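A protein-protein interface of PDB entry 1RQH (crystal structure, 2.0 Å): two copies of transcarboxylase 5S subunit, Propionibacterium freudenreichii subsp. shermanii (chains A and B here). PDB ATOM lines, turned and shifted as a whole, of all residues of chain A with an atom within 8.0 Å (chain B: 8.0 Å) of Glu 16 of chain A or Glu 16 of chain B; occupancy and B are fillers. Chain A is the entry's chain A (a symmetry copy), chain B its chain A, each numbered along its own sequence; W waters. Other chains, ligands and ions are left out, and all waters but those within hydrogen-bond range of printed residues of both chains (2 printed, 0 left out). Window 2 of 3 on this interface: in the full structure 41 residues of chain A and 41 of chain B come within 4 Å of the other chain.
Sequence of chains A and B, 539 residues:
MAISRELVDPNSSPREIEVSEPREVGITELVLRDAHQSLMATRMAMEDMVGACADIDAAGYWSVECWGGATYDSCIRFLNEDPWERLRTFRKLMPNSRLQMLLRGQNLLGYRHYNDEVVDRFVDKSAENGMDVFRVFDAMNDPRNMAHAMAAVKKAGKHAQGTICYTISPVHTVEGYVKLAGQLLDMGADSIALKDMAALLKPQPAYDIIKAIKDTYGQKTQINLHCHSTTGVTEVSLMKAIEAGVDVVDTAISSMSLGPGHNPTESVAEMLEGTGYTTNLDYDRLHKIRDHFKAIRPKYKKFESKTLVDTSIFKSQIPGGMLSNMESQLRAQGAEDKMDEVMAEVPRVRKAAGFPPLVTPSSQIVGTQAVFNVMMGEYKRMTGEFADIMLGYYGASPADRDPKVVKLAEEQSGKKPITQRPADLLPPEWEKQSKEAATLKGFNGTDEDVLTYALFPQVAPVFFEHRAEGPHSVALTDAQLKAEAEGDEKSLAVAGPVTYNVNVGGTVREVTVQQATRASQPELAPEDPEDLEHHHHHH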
ATOM      1  N   ARG A  15       4.166 -20.524 -22.794  1.00  0.00           N
ATOM      2  CA  ARG A  15       4.227 -20.435 -24.284  1.00  0.00           C
ATOM      3  C   ARG A  15       5.451 -19.593 -24.658  1.00  0.00           C
ATOM      4  O   ARG A  15       5.585 -18.452 -24.213  1.00  0.00           O
ATOM      5  CB  ARG A  15       2.942 -19.786 -24.804  1.00  0.00           C
ATOM      6  CG  ARG A  15       2.734 -20.074 -26.146  1.00  0.00           C
ATOM      7  CD  ARG A  15       1.572 -19.465 -26.605  1.00  0.00           C
ATOM      8  NE  ARG A  15       1.348 -19.707 -28.029  1.00  0.00           N
ATOM      9  CZ  ARG A  15       0.877 -18.797 -28.877  1.00  0.00           C
ATOM     10  NH1 ARG A  15       0.576 -17.581 -28.448  1.00  0.00           N
ATOM     11  NH2 ARG A  15       0.721 -19.100 -30.161  1.00  0.00           N
ATOM     12  N   GLU A  16       6.346 -20.146 -25.471  1.00  0.00           N
ATOM     13  CA  GLU A  16       7.557 -19.417 -25.826  1.00  0.00           C
ATOM     14  C   GLU A  16       7.857 -19.525 -27.314  1.00  0.00           C
ATOM     15  O   GLU A  16       7.386 -20.430 -28.001  1.00  0.00           O
ATOM     16  CB  GLU A  16       8.735 -19.992 -25.052  1.00  0.00           C
ATOM     17  CG  GLU A  16       8.462 -20.026 -23.690  1.00  0.00           C
ATOM     18  CD  GLU A  16       9.692 -19.780 -22.860  1.00  0.00           C
ATOM     19  OE1 GLU A  16      10.003 -18.595 -22.595  1.00  0.00           O
ATOM     20  OE2 GLU A  16      10.354 -20.771 -22.485  1.00  0.00           O
ATOM     21  N   ILE A  17       8.663 -18.583 -27.796  1.00  0.00           N
ATOM     22  CA  ILE A  17       9.094 -18.563 -29.184  1.00  0.00           C
ATOM     23  C   ILE A  17      10.609 -18.400 -29.217  1.00  0.00           C
ATOM     24  O   ILE A  17      11.160 -17.472 -28.625  1.00  0.00           O
ATOM     25  CB  ILE A  17       8.476 -17.391 -29.965  1.00  0.00           C
ATOM     26  CG1 ILE A  17       6.968 -17.580 -30.093  1.00  0.00           C
ATOM     27  CG2 ILE A  17       9.118 -17.300 -31.343  1.00  0.00           C
ATOM     28  CD1 ILE A  17       6.283 -16.434 -30.797  1.00  0.00           C
ATOM     29  N   GLU A  18      11.287 -19.313 -29.894  1.00  0.00           N
ATOM     30  CA  GLU A  18      12.730 -19.229 -29.994  1.00  0.00           C
ATOM     31  C   GLU A  18      13.097 -18.122 -30.970  1.00  0.00           C
ATOM     32  O   GLU A  18      12.520 -18.031 -32.056  1.00  0.00           O
ATOM     33  CB  GLU A  18      13.288 -20.567 -30.480  1.00  0.00           C
ATOM     34  CG  GLU A  18      14.659 -20.477 -30.695  1.00  0.00           C
ATOM     35  CD  GLU A  18      15.293 -21.811 -31.008  1.00  0.00           C
ATOM     36  OE1 GLU A  18      15.835 -22.437 -30.076  1.00  0.00           O
ATOM     37  OE2 GLU A  18      15.237 -22.238 -32.179  1.00  0.00           O
ATOM     38  N   VAL A  19      14.042 -17.271 -30.586  1.00  0.00           N
ATOM     39  CA  VAL A  19      14.478 -16.188 -31.464  1.00  0.00           C
ATOM     40  C   VAL A  19      15.991 -16.256 -31.620  1.00  0.00           C
ATOM     41  O   VAL A  19      16.683 -16.758 -30.728  1.00  0.00           O
ATOM     42  CB  VAL A  19      14.069 -14.816 -30.902  1.00  0.00           C
ATOM     43  CG1 VAL A  19      12.549 -14.727 -30.841  1.00  0.00           C
ATOM     44  CG2 VAL A  19      14.681 -14.611 -29.524  1.00  0.00           C
ATOM     45  N   SER A  20      16.505 -15.761 -32.747  1.00  0.00           N
ATOM     46  CA  SER A  20      17.940 -15.792 -33.029  1.00  0.00           C
ATOM     47  C   SER A  20      18.689 -14.946 -32.003  1.00  0.00           C
ATOM     48  O   SER A  20      18.113 -14.053 -31.382  1.00  0.00           O
ATOM     49  CB  SER A  20      18.202 -15.275 -34.449  1.00  0.00           C
ATOM     50  OG  SER A  20      17.699 -13.961 -34.619  1.00  0.00           O
ATOM     51  N   TYR A 207       8.504 -16.384 -40.453  1.00  0.00           N
ATOM     52  CA  TYR A 207       9.296 -17.009 -39.405  1.00  0.00           C
ATOM     53  C   TYR A 207       9.540 -18.490 -39.734  1.00  0.00           C
ATOM     54  O   TYR A 207      10.676 -18.953 -39.707  1.00  0.00           O
ATOM     55  CB  TYR A 207       8.547 -16.912 -38.068  1.00  0.00           C
ATOM     56  CG  TYR A 207       9.266 -17.599 -36.919  1.00  0.00           C
ATOM     57  CD1 TYR A 207      10.162 -16.899 -36.107  1.00  0.00           C
ATOM     58  CD2 TYR A 207       9.065 -18.958 -36.658  1.00  0.00           C
ATOM     59  CE1 TYR A 207      10.837 -17.539 -35.064  1.00  0.00           C
ATOM     60  CE2 TYR A 207       9.740 -19.607 -35.620  1.00  0.00           C
ATOM     61  CZ  TYR A 207      10.618 -18.891 -34.829  1.00  0.00           C
ATOM     62  OH  TYR A 207      11.261 -19.522 -33.792  1.00  0.00           O
ATOM     63  N   ARG B  15      17.760 -18.902 -26.945  1.00  0.00           N
ATOM     64  CA  ARG B  15      17.147 -17.561 -26.699  1.00  0.00           C
ATOM     65  C   ARG B  15      15.643 -17.673 -26.961  1.00  0.00           C
ATOM     66  O   ARG B  15      15.224 -18.076 -28.047  1.00  0.00           O
ATOM     67  CB  ARG B  15      17.788 -16.535 -27.637  1.00  0.00           C
ATOM     68  CG  ARG B  15      17.607 -15.239 -27.171  1.00  0.00           C
ATOM     69  CD  ARG B  15      18.180 -14.320 -28.042  1.00  0.00           C
ATOM     70  NE  ARG B  15      17.967 -12.941 -27.607  1.00  0.00           N
ATOM     71  CZ  ARG B  15      17.699 -11.931 -28.430  1.00  0.00           C
ATOM     72  NH1 ARG B  15      17.613 -12.140 -29.735  1.00  0.00           N
ATOM     73  NH2 ARG B  15      17.501 -10.710 -27.945  1.00  0.00           N
ATOM     74  N   GLU B  16      14.825 -17.319 -25.974  1.00  0.00           N
ATOM     75  CA  GLU B  16      13.382 -17.448 -26.141  1.00  0.00           C
ATOM     76  C   GLU B  16      12.649 -16.215 -25.632  1.00  0.00           C
ATOM     77  O   GLU B  16      13.171 -15.442 -24.830  1.00  0.00           O
ATOM     78  CB  GLU B  16      12.892 -18.659 -25.361  1.00  0.00           C
ATOM     79  CG  GLU B  16      13.615 -19.794 -25.705  1.00  0.00           C
ATOM     80  CD  GLU B  16      12.770 -21.038 -25.668  1.00  0.00           C
ATOM     81  OE1 GLU B  16      12.121 -21.346 -26.694  1.00  0.00           O
ATOM     82  OE2 GLU B  16      12.743 -21.697 -24.606  1.00  0.00           O
ATOM     83  N   ILE B  17      11.419 -16.054 -26.109  1.00  0.00           N
ATOM     84  CA  ILE B  17      10.559 -14.959 -25.692  1.00  0.00           C
ATOM     85  C   ILE B  17       9.201 -15.533 -25.300  1.00  0.00           C
ATOM     86  O   ILE B  17       8.569 -16.251 -26.076  1.00  0.00           O
ATOM     87  CB  ILE B  17      10.332 -13.939 -26.819  1.00  0.00           C
ATOM     88  CG1 ILE B  17      11.637 -13.222 -27.150  1.00  0.00           C
ATOM     89  CG2 ILE B  17       9.269 -12.935 -26.394  1.00  0.00           C
ATOM     90  CD1 ILE B  17      11.504 -12.245 -28.294  1.00  0.00           C
ATOM     91  N   GLU B  18       8.759 -15.235 -24.089  1.00  0.00           N
ATOM     92  CA  GLU B  18       7.472 -15.723 -23.638  1.00  0.00           C
ATOM     93  C   GLU B  18       6.371 -14.924 -24.319  1.00  0.00           C
ATOM     94  O   GLU B  18       6.439 -13.695 -24.383  1.00  0.00           O
ATOM     95  CB  GLU B  18       7.372 -15.570 -22.120  1.00  0.00           C
ATOM     96  CG  GLU B  18       6.102 -15.924 -21.676  1.00  0.00           C
ATOM     97  CD  GLU B  18       5.996 -15.960 -20.171  1.00  0.00           C
ATOM     98  OE1 GLU B  18       6.118 -17.062 -19.599  1.00  0.00           O
ATOM     99  OE2 GLU B  18       5.803 -14.890 -19.559  1.00  0.00           O
ATOM    100  N   VAL B  19       5.365 -15.615 -24.843  1.00  0.00           N
ATOM    101  CA  VAL B  19       4.251 -14.936 -25.499  1.00  0.00           C
ATOM    102  C   VAL B  19       2.945 -15.408 -24.872  1.00  0.00           C
ATOM    103  O   VAL B  19       2.877 -16.528 -24.354  1.00  0.00           O
ATOM    104  CB  VAL B  19       4.239 -15.215 -27.011  1.00  0.00           C
ATOM    105  CG1 VAL B  19       5.508 -14.653 -27.640  1.00  0.00           C
ATOM    106  CG2 VAL B  19       4.124 -16.712 -27.266  1.00  0.00           C
ATOM    107  N   SER B  20       1.915 -14.562 -24.913  1.00  0.00           N
ATOM    108  CA  SER B  20       0.617 -14.886 -24.322  1.00  0.00           C
ATOM    109  C   SER B  20       0.003 -16.084 -25.042  1.00  0.00           C
ATOM    110  O   SER B  20       0.347 -16.374 -26.188  1.00  0.00           O
ATOM    111  CB  SER B  20      -0.313 -13.669 -24.411  1.00  0.00           C
ATOM    112  OG  SER B  20      -0.479 -13.245 -25.753  1.00  0.00           O
ATOM    113  N   TYR B 207       6.212  -4.320 -25.577  1.00  0.00           N
ATOM    114  CA  TYR B 207       6.166  -5.629 -24.942  1.00  0.00           C
ATOM    115  C   TYR B 207       6.441  -5.500 -23.437  1.00  0.00           C
ATOM    116  O   TYR B 207       5.679  -6.007 -22.619  1.00  0.00           O
ATOM    117  CB  TYR B 207       7.228  -6.543 -25.568  1.00  0.00           C
ATOM    118  CG  TYR B 207       7.304  -7.917 -24.925  1.00  0.00           C
ATOM    119  CD1 TYR B 207       6.550  -8.986 -25.415  1.00  0.00           C
ATOM    120  CD2 TYR B 207       8.113  -8.141 -23.807  1.00  0.00           C
ATOM    121  CE1 TYR B 207       6.605 -10.243 -24.807  1.00  0.00           C
ATOM    122  CE2 TYR B 207       8.171  -9.394 -23.190  1.00  0.00           C
ATOM    123  CZ  TYR B 207       7.418 -10.436 -23.697  1.00  0.00           C
ATOM    124  OH  TYR B 207       7.496 -11.674 -23.108  1.00  0.00           O
HETATM  125  O   HOH W   1       2.278 -18.109 -21.901  1.00  0.00           O
HETATM  126  O   HOH W   2      18.692 -18.835 -29.998  1.00  0.00           O
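The backbone NH of Ile 17 of chain B is in hydrogen-bond range of the backbone carbonyl oxygen of Ile 17 of chain A (2.9 Å). O of Ser 20 of chain A is in hydrogen-bond range of NH1 of Arg 15 of chain B, 2.6 Å away. O of Arg 15 of chain B sits at hydrogen-bond distance from N of Val 19 of chain A. N of Val 19 of chain B sits at hydrogen-bond distance from O of Arg 15 of chain A, at 2.9 Å. OE2 of Glu 16 of chain A lies close to OE2 of Glu 16 of chain B, at 3.3 Å. NH1 of Arg 15 of chain A is in hydrogen-bond range of O of Ser 20 of chain B.
O of Glu 18 of chain B is in hydrogen-bond range of OH of Tyr 207 of chain B (2.6 Å). OH of Tyr 207 of chain A lies within hydrogen-bond range of O of Glu 18 of chain A (2.6 Å).
Among the printed residues, merely in contact across the chains: Arg 15 of chain A with Glu 18 of chain B (3.4 Å), Glu 16 of chain A with Ile 17 of chain B (3.3 Å), Glu 16 of chain A with Glu 18 of chain B (3.9 Å), Ile 17 of chain A with Glu 16 of chain B (3.3 Å), Ile 17 of chain A with Val 19 of chain B (3.7 Å), Glu 18 of chain A with Arg 15 of chain B (3.4 Å), Glu 18 of chain A with Glu 16 of chain B (3.9 Å) and Val 19 of chain A with Ile 17 of chain B (3.7 Å).
Printed residues of chain B within 4 Å of Glu 16 of chain A: Glu 16, Ile 17 and Glu 18. Glu 16 of chain B touches just these residues of chain A: Glu 16, Ile 17 and Glu 18. Printed residues of chain A within 4 Å of Val 19 of chain B: Arg 15 and Ile 17. Of the printed residues of chain B, Ile 17 of chain A touches Glu 16, Ile 17 and Val 19. Tyr 207 of chain B touches none of the printed residues of chain A. The nearest residue of chain B that does not touch Glu 16 of chain A is Val 19 of chain B (4.5 Å). The nearest residue of chain A that does not touch Glu 16 of chain B is Val 19 of chain A (4.5 Å).
Among the printed residues, 14 pairs touch across the chains.
Arg 15 of chain A touches Val 19 of chain B, and with the chains exchanged Val 19 of chain A touches Arg 15 of chain B. Arg 15 of chain A touches Ser 20 of chain B, and with the chains exchanged Ser 20 of chain A touches Arg 15 of chain B. Glu 16 of chain A touches Ile 17 of chain B, and with the chains exchanged Ile 17 of chain A touches Glu 16 of chain B. Ile 17 of chain A touches its own counterpart, Ile 17 of chain B.
Water W1 bridges O of Val 19 of chain B (3.0 Å) and N of Arg 15 of chain A (3.2 Å). Water W2 bridges the backbone carbonyl oxygen of Val 19 of chain A (3.0 Å) and the backbone NH of Arg 15 of chain B (3.2 Å).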
